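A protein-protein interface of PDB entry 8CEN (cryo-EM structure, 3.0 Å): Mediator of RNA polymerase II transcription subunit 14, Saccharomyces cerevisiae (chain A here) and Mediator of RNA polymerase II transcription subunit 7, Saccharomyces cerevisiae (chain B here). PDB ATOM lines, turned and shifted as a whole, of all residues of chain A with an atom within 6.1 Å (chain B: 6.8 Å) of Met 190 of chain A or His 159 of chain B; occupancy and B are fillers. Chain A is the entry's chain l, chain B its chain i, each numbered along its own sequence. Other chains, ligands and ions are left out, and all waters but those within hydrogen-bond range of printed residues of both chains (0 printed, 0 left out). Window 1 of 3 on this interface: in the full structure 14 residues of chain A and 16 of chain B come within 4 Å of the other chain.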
ATOM      1  N   SER A 185     -11.406  23.277   1.100  1.00  0.00           N
ATOM      2  CA  SER A 185     -11.781  23.755   2.427  1.00  0.00           C
ATOM      3  C   SER A 185     -12.948  22.951   2.986  1.00  0.00           C
ATOM      4  O   SER A 185     -13.006  22.681   4.191  1.00  0.00           O
ATOM      5  CB  SER A 185     -12.130  25.241   2.379  1.00  0.00           C
ATOM      6  OG  SER A 185     -13.126  25.496   1.409  1.00  0.00           O
ATOM      7  N   SER A 186     -13.881  22.553   2.115  1.00  0.00           N
ATOM      8  CA  SER A 186     -14.955  21.657   2.534  1.00  0.00           C
ATOM      9  C   SER A 186     -14.407  20.295   2.951  1.00  0.00           C
ATOM     10  O   SER A 186     -14.930  19.665   3.877  1.00  0.00           O
ATOM     11  CB  SER A 186     -15.974  21.506   1.407  1.00  0.00           C
ATOM     12  OG  SER A 186     -16.496  22.767   1.025  1.00  0.00           O
ATOM     13  N   LEU A 187     -13.367  19.821   2.262  1.00  0.00           N
ATOM     14  CA  LEU A 187     -12.682  18.590   2.656  1.00  0.00           C
ATOM     15  C   LEU A 187     -12.027  18.731   4.025  1.00  0.00           C
ATOM     16  O   LEU A 187     -12.144  17.845   4.878  1.00  0.00           O
ATOM     17  CB  LEU A 187     -11.632  18.225   1.606  1.00  0.00           C
ATOM     18  CG  LEU A 187     -12.033  17.334   0.435  1.00  0.00           C
ATOM     19  CD1 LEU A 187     -11.014  17.444  -0.684  1.00  0.00           C
ATOM     20  CD2 LEU A 187     -12.116  15.907   0.924  1.00  0.00           C
ATOM     21  N   ASN A 188     -11.322  19.843   4.245  1.00  0.00           N
ATOM     22  CA  ASN A 188     -10.628  20.067   5.508  1.00  0.00           C
ATOM     23  C   ASN A 188     -11.591  20.308   6.660  1.00  0.00           C
ATOM     24  O   ASN A 188     -11.218  20.095   7.819  1.00  0.00           O
ATOM     25  CB  ASN A 188      -9.663  21.245   5.379  1.00  0.00           C
ATOM     26  CG  ASN A 188      -8.619  21.022   4.305  1.00  0.00           C
ATOM     27  OD1 ASN A 188      -8.108  19.914   4.142  1.00  0.00           O
ATOM     28  ND2 ASN A 188      -8.292  22.077   3.567  1.00  0.00           N
ATOM     29  N   SER A 189     -12.814  20.749   6.365  1.00  0.00           N
ATOM     30  CA  SER A 189     -13.842  20.878   7.389  1.00  0.00           C
ATOM     31  C   SER A 189     -14.302  19.532   7.934  1.00  0.00           C
ATOM     32  O   SER A 189     -14.902  19.488   9.013  1.00  0.00           O
ATOM     33  CB  SER A 189     -15.044  21.636   6.824  1.00  0.00           C
ATOM     34  OG  SER A 189     -16.083  21.729   7.783  1.00  0.00           O
ATOM     35  N   MET A 190     -14.035  18.441   7.221  1.00  0.00           N
ATOM     36  CA  MET A 190     -14.573  17.131   7.558  1.00  0.00           C
ATOM     37  C   MET A 190     -13.655  16.322   8.463  1.00  0.00           C
ATOM     38  O   MET A 190     -14.024  15.209   8.849  1.00  0.00           O
ATOM     39  CB  MET A 190     -14.837  16.341   6.278  1.00  0.00           C
ATOM     40  CG  MET A 190     -15.896  16.977   5.425  1.00  0.00           C
ATOM     41  SD  MET A 190     -17.527  17.061   6.159  1.00  0.00           S
ATOM     42  CE  MET A 190     -18.301  18.077   4.915  1.00  0.00           C
ATOM     43  N   THR A 191     -12.471  16.845   8.796  1.00  0.00           N
ATOM     44  CA  THR A 191     -11.486  16.056   9.531  1.00  0.00           C
ATOM     45  C   THR A 191     -11.944  15.788  10.961  1.00  0.00           C
ATOM     46  O   THR A 191     -11.861  14.655  11.448  1.00  0.00           O
ATOM     47  CB  THR A 191     -10.131  16.767   9.521  1.00  0.00           C
ATOM     48  OG1 THR A 191     -10.247  18.038  10.171  1.00  0.00           O
ATOM     49  CG2 THR A 191      -9.670  16.987   8.092  1.00  0.00           C
ATOM     50  N   ASN A 192     -12.441  16.816  11.643  1.00  0.00           N
ATOM     51  CA  ASN A 192     -12.945  16.632  12.995  1.00  0.00           C
ATOM     52  C   ASN A 192     -14.324  15.982  13.011  1.00  0.00           C
ATOM     53  O   ASN A 192     -14.702  15.376  14.021  1.00  0.00           O
ATOM     54  CB  ASN A 192     -12.979  17.987  13.711  1.00  0.00           C
ATOM     55  CG  ASN A 192     -13.536  17.901  15.118  1.00  0.00           C
ATOM     56  OD1 ASN A 192     -14.225  18.809  15.577  1.00  0.00           O
ATOM     57  ND2 ASN A 192     -13.216  16.819  15.820  1.00  0.00           N
ATOM     58  N   ALA A 193     -15.058  16.035  11.905  1.00  0.00           N
ATOM     59  CA  ALA A 193     -16.464  15.649  11.886  1.00  0.00           C
ATOM     60  C   ALA A 193     -16.579  14.210  11.396  1.00  0.00           C
ATOM     61  O   ALA A 193     -16.927  13.943  10.246  1.00  0.00           O
ATOM     62  CB  ALA A 193     -17.239  16.586  11.017  1.00  0.00           C
ATOM     63  N   LYS A 194     -16.287  13.278  12.299  1.00  0.00           N
ATOM     64  CA  LYS A 194     -16.576  11.860  12.133  1.00  0.00           C
ATOM     65  C   LYS A 194     -17.040  11.331  13.482  1.00  0.00           C
ATOM     66  O   LYS A 194     -17.256  12.091  14.432  1.00  0.00           O
ATOM     67  CB  LYS A 194     -15.363  11.060  11.628  1.00  0.00           C
ATOM     68  CG  LYS A 194     -14.624  11.621  10.426  1.00  0.00           C
ATOM     69  CD  LYS A 194     -15.248  11.126   9.136  1.00  0.00           C
ATOM     70  CE  LYS A 194     -15.040  12.120   8.008  1.00  0.00           C
ATOM     71  NZ  LYS A 194     -13.604  12.386   7.751  1.00  0.00           N
ATOM     72  N   LEU B  89     -25.576  13.072  20.844  1.00  0.00           N
ATOM     73  CA  LEU B  89     -25.194  13.544  19.520  1.00  0.00           C
ATOM     74  C   LEU B  89     -25.942  14.830  19.191  1.00  0.00           C
ATOM     75  O   LEU B  89     -27.180  14.830  19.181  1.00  0.00           O
ATOM     76  CB  LEU B  89     -25.482  12.475  18.473  1.00  0.00           C
ATOM     77  CG  LEU B  89     -24.936  12.770  17.079  1.00  0.00           C
ATOM     78  CD1 LEU B  89     -23.423  12.757  17.105  1.00  0.00           C
ATOM     79  CD2 LEU B  89     -25.453  11.758  16.081  1.00  0.00           C
ATOM     80  N   LEU B 119     -29.662   7.468   3.526  1.00  0.00           N
ATOM     81  CA  LEU B 119     -28.245   7.496   3.180  1.00  0.00           C
ATOM     82  C   LEU B 119     -28.031   7.224   1.696  1.00  0.00           C
ATOM     83  O   LEU B 119     -27.193   7.873   1.057  1.00  0.00           O
ATOM     84  CB  LEU B 119     -27.493   6.481   4.036  1.00  0.00           C
ATOM     85  CG  LEU B 119     -25.972   6.571   4.125  1.00  0.00           C
ATOM     86  CD1 LEU B 119     -25.545   7.916   4.681  1.00  0.00           C
ATOM     87  CD2 LEU B 119     -25.465   5.446   5.005  1.00  0.00           C
ATOM     88  N   LEU B 122     -29.098  10.355  -0.079  1.00  0.00           N
ATOM     89  CA  LEU B 122     -28.101  11.401   0.107  1.00  0.00           C
ATOM     90  C   LEU B 122     -26.874  11.162  -0.766  1.00  0.00           C
ATOM     91  O   LEU B 122     -26.297  12.112  -1.302  1.00  0.00           O
ATOM     92  CB  LEU B 122     -27.712  11.477   1.582  1.00  0.00           C
ATOM     93  CG  LEU B 122     -28.567  12.353   2.499  1.00  0.00           C
ATOM     94  CD1 LEU B 122     -28.279  12.032   3.954  1.00  0.00           C
ATOM     95  CD2 LEU B 122     -28.324  13.820   2.226  1.00  0.00           C
ATOM     96  N   ILE B 151     -23.190  20.890  -1.686  1.00  0.00           N
ATOM     97  CA  ILE B 151     -22.349  19.711  -1.488  1.00  0.00           C
ATOM     98  C   ILE B 151     -21.869  19.639  -0.037  1.00  0.00           C
ATOM     99  O   ILE B 151     -21.823  18.561   0.569  1.00  0.00           O
ATOM    100  CB  ILE B 151     -21.186  19.731  -2.498  1.00  0.00           C
ATOM    101  CG1 ILE B 151     -21.736  19.498  -3.906  1.00  0.00           C
ATOM    102  CG2 ILE B 151     -20.151  18.671  -2.180  1.00  0.00           C
ATOM    103  CD1 ILE B 151     -20.741  19.742  -5.007  1.00  0.00           C
ATOM    104  N   ARG B 152     -21.563  20.800   0.548  1.00  0.00           N
ATOM    105  CA  ARG B 152     -21.142  20.916   1.943  1.00  0.00           C
ATOM    106  C   ARG B 152     -22.238  20.443   2.905  1.00  0.00           C
ATOM    107  O   ARG B 152     -21.980  19.636   3.812  1.00  0.00           O
ATOM    108  CB  ARG B 152     -20.732  22.386   2.149  1.00  0.00           C
ATOM    109  CG  ARG B 152     -20.101  22.950   3.436  1.00  0.00           C
ATOM    110  CD  ARG B 152     -21.134  23.537   4.386  1.00  0.00           C
ATOM    111  NE  ARG B 152     -20.515  24.138   5.564  1.00  0.00           N
ATOM    112  CZ  ARG B 152     -20.169  23.493   6.667  1.00  0.00           C
ATOM    113  NH1 ARG B 152     -20.373  22.196   6.802  1.00  0.00           N
ATOM    114  NH2 ARG B 152     -19.609  24.171   7.663  1.00  0.00           N
ATOM    115  N   THR B 153     -23.486  20.868   2.674  1.00  0.00           N
ATOM    116  CA  THR B 153     -24.562  20.420   3.555  1.00  0.00           C
ATOM    117  C   THR B 153     -24.986  18.974   3.288  1.00  0.00           C
ATOM    118  O   THR B 153     -25.349  18.267   4.237  1.00  0.00           O
ATOM    119  CB  THR B 153     -25.779  21.353   3.491  1.00  0.00           C
ATOM    120  OG1 THR B 153     -26.820  20.830   4.327  1.00  0.00           O
ATOM    121  CG2 THR B 153     -26.319  21.491   2.098  1.00  0.00           C
ATOM    122  N   ILE B 154     -24.918  18.503   2.037  1.00  0.00           N
ATOM    123  CA  ILE B 154     -25.193  17.096   1.746  1.00  0.00           C
ATOM    124  C   ILE B 154     -24.173  16.203   2.446  1.00  0.00           C
ATOM    125  O   ILE B 154     -24.526  15.175   3.042  1.00  0.00           O
ATOM    126  CB  ILE B 154     -25.201  16.853   0.222  1.00  0.00           C
ATOM    127  CG1 ILE B 154     -26.493  17.366  -0.421  1.00  0.00           C
ATOM    128  CG2 ILE B 154     -25.013  15.378  -0.094  1.00  0.00           C
ATOM    129  CD1 ILE B 154     -27.659  16.440  -0.272  1.00  0.00           C
ATOM    130  N   LEU B 155     -22.896  16.595   2.409  1.00  0.00           N
ATOM    131  CA  LEU B 155     -21.851  15.809   3.051  1.00  0.00           C
ATOM    132  C   LEU B 155     -21.978  15.812   4.568  1.00  0.00           C
ATOM    133  O   LEU B 155     -21.788  14.766   5.200  1.00  0.00           O
ATOM    134  CB  LEU B 155     -20.475  16.313   2.634  1.00  0.00           C
ATOM    135  CG  LEU B 155     -20.042  15.813   1.267  1.00  0.00           C
ATOM    136  CD1 LEU B 155     -18.794  16.536   0.791  1.00  0.00           C
ATOM    137  CD2 LEU B 155     -19.815  14.313   1.384  1.00  0.00           C
ATOM    138  N   VAL B 156     -22.289  16.963   5.181  1.00  0.00           N
ATOM    139  CA  VAL B 156     -22.450  16.926   6.635  1.00  0.00           C
ATOM    140  C   VAL B 156     -23.703  16.152   7.024  1.00  0.00           C
ATOM    141  O   VAL B 156     -23.750  15.543   8.097  1.00  0.00           O
ATOM    142  CB  VAL B 156     -22.446  18.331   7.275  1.00  0.00           C
ATOM    143  CG1 VAL B 156     -21.133  19.015   7.027  1.00  0.00           C
ATOM    144  CG2 VAL B 156     -23.613  19.186   6.825  1.00  0.00           C
ATOM    145  N   ASN B 157     -24.729  16.139   6.167  1.00  0.00           N
ATOM    146  CA  ASN B 157     -25.890  15.302   6.438  1.00  0.00           C
ATOM    147  C   ASN B 157     -25.544  13.820   6.351  1.00  0.00           C
ATOM    148  O   ASN B 157     -26.007  13.022   7.177  1.00  0.00           O
ATOM    149  CB  ASN B 157     -27.012  15.649   5.467  1.00  0.00           C
ATOM    150  CG  ASN B 157     -27.797  16.863   5.899  1.00  0.00           C
ATOM    151  OD1 ASN B 157     -28.930  16.741   6.355  1.00  0.00           O
ATOM    152  ND2 ASN B 157     -27.201  18.042   5.765  1.00  0.00           N
ATOM    153  N   ILE B 158     -24.724  13.439   5.367  1.00  0.00           N
ATOM    154  CA  ILE B 158     -24.266  12.054   5.248  1.00  0.00           C
ATOM    155  C   ILE B 158     -23.473  11.653   6.485  1.00  0.00           C
ATOM    156  O   ILE B 158     -23.712  10.599   7.091  1.00  0.00           O
ATOM    157  CB  ILE B 158     -23.427  11.878   3.968  1.00  0.00           C
ATOM    158  CG1 ILE B 158     -24.323  11.880   2.732  1.00  0.00           C
ATOM    159  CG2 ILE B 158     -22.604  10.595   4.025  1.00  0.00           C
ATOM    160  CD1 ILE B 158     -23.568  11.980   1.432  1.00  0.00           C
ATOM    161  N   HIS B 159     -22.543  12.516   6.898  1.00  0.00           N
ATOM    162  CA  HIS B 159     -21.696  12.208   8.045  1.00  0.00           C
ATOM    163  C   HIS B 159     -22.500  12.170   9.341  1.00  0.00           C
ATOM    164  O   HIS B 159     -22.249  11.322  10.203  1.00  0.00           O
ATOM    165  CB  HIS B 159     -20.552  13.216   8.136  1.00  0.00           C
ATOM    166  CG  HIS B 159     -19.500  13.030   7.086  1.00  0.00           C
ATOM    167  ND1 HIS B 159     -19.539  13.673   5.867  1.00  0.00           N
ATOM    168  CD2 HIS B 159     -18.398  12.245   7.059  1.00  0.00           C
ATOM    169  CE1 HIS B 159     -18.494  13.311   5.146  1.00  0.00           C
ATOM    170  NE2 HIS B 159     -17.787  12.442   5.845  1.00  0.00           N
ATOM    171  N   HIS B 160     -23.494  13.052   9.485  1.00  0.00           N
ATOM    172  CA  HIS B 160     -24.335  13.029  10.674  1.00  0.00           C
ATOM    173  C   HIS B 160     -25.237  11.806  10.709  1.00  0.00           C
ATOM    174  O   HIS B 160     -25.520  11.284  11.791  1.00  0.00           O
ATOM    175  CB  HIS B 160     -25.184  14.294  10.757  1.00  0.00           C
ATOM    176  CG  HIS B 160     -25.784  14.522  12.108  1.00  0.00           C
ATOM    177  ND1 HIS B 160     -27.016  14.020  12.471  1.00  0.00           N
ATOM    178  CD2 HIS B 160     -25.321  15.196  13.185  1.00  0.00           C
ATOM    179  CE1 HIS B 160     -27.284  14.377  13.714  1.00  0.00           C
ATOM    180  NE2 HIS B 160     -26.271  15.092  14.171  1.00  0.00           N
ATOM    181  N   LEU B 161     -25.709  11.343   9.549  1.00  0.00           N
ATOM    182  CA  LEU B 161     -26.473  10.100   9.509  1.00  0.00           C
ATOM    183  C   LEU B 161     -25.602   8.910   9.897  1.00  0.00           C
ATOM    184  O   LEU B 161     -26.057   8.004  10.610  1.00  0.00           O
ATOM    185  CB  LEU B 161     -27.082   9.914   8.119  1.00  0.00           C
ATOM    186  CG  LEU B 161     -28.341   9.057   7.991  1.00  0.00           C
ATOM    187  CD1 LEU B 161     -29.419   9.536   8.941  1.00  0.00           C
ATOM    188  CD2 LEU B 161     -28.846   9.102   6.560  1.00  0.00           C
ATOM    189  N   LEU B 162     -24.337   8.910   9.462  1.00  0.00           N
ATOM    190  CA  LEU B 162     -23.405   7.878   9.912  1.00  0.00           C
ATOM    191  C   LEU B 162     -23.179   7.950  11.420  1.00  0.00           C
ATOM    192  O   LEU B 162     -23.085   6.917  12.091  1.00  0.00           O
ATOM    193  CB  LEU B 162     -22.074   7.992   9.174  1.00  0.00           C
ATOM    194  CG  LEU B 162     -22.119   7.871   7.652  1.00  0.00           C
ATOM    195  CD1 LEU B 162     -20.743   8.079   7.040  1.00  0.00           C
ATOM    196  CD2 LEU B 162     -22.713   6.547   7.230  1.00  0.00           C
ATOM    197  N   ASN B 163     -23.094   9.162  11.972  1.00  0.00           N
ATOM    198  CA  ASN B 163     -22.904   9.300  13.414  1.00  0.00           C
ATOM    199  C   ASN B 163     -24.147   8.888  14.198  1.00  0.00           C
ATOM    200  O   ASN B 163     -24.028   8.401  15.328  1.00  0.00           O
ATOM    201  CB  ASN B 163     -22.504  10.733  13.758  1.00  0.00           C
ATOM    202  CG  ASN B 163     -21.257  11.172  13.027  1.00  0.00           C
ATOM    203  OD1 ASN B 163     -20.474  10.346  12.566  1.00  0.00           O
ATOM    204  ND2 ASN B 163     -21.073  12.478  12.897  1.00  0.00           N
ATOM    205  N   GLU B 164     -25.339   9.093  13.632  1.00  0.00           N
ATOM    206  CA  GLU B 164     -26.555   8.573  14.252  1.00  0.00           C
ATOM    207  C   GLU B 164     -26.580   7.052  14.218  1.00  0.00           C
ATOM    208  O   GLU B 164     -27.066   6.412  15.158  1.00  0.00           O
ATOM    209  CB  GLU B 164     -27.795   9.133  13.556  1.00  0.00           C
ATOM    210  CG  GLU B 164     -28.015  10.620  13.732  1.00  0.00           C
ATOM    211  CD  GLU B 164     -29.248  11.111  13.003  1.00  0.00           C
ATOM    212  OE1 GLU B 164     -29.855  10.310  12.262  1.00  0.00           O
ATOM    213  OE2 GLU B 164     -29.608  12.295  13.167  1.00  0.00           O
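Met 190 of chain A touches just these residues of chain B: Leu 155 (3.6 Å), Val 156 (3.7 Å) and His 159 (3.95 Å). His 159 of chain B touches just these residues of chain A: Met 190 (3.95 Å), Ala 193 (3.9 Å) and Lys 194 (3.5 Å). Printed residues of chain B within 4 Å of Lys 194 of chain A: His 159 (3.5 Å) and Asn 163 (3.7 Å). Of the printed residues of chain A, Val 156 of chain B touches Met 190. Leu 119 of chain B touches none of the printed residues of chain A.
Among the printed residues, merely in contact across the chains: Lys 194 of chain A with His 159 of chain B (3.5 Å), Met 190 of chain A with Leu 155 of chain B (3.6 Å), Met 190 of chain A with Val 156 of chain B (3.7 Å), Lys 194 of chain A with Asn 163 of chain B (3.7 Å), Ala 193 of chain A with His 159 of chain B (3.9 Å) and Met 190 of chain A with His 159 of chain B (3.95 Å).
Along chain A the printed residues that touch a printed residue of chain B span positions 190 to 194. Hydrophobic or aromatic side chains of chain B that line the printed part of chain A: Leu 155, Val 156 and His 159. Along chain B the printed residues that touch a printed residue of chain A span positions 155 to 163. Among the printed residues, no Asp or Glu carboxylate lies within 4 Å of a Lys or Arg side-chain nitrogen of the other chain.
O of Met 190 of chain A lies within hydrogen-bond range of NZ of Lys 194 of chain A, 3.1 Å away. The backbone carbonyl oxygen of Leu 155 of chain B lies within hydrogen-bond range of a ring nitrogen (ND1) of His 159 of chain B (2.6 Å). O of His 159 of chain B lies close to OD1 of Asn 163 of chain B (3.1 Å).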
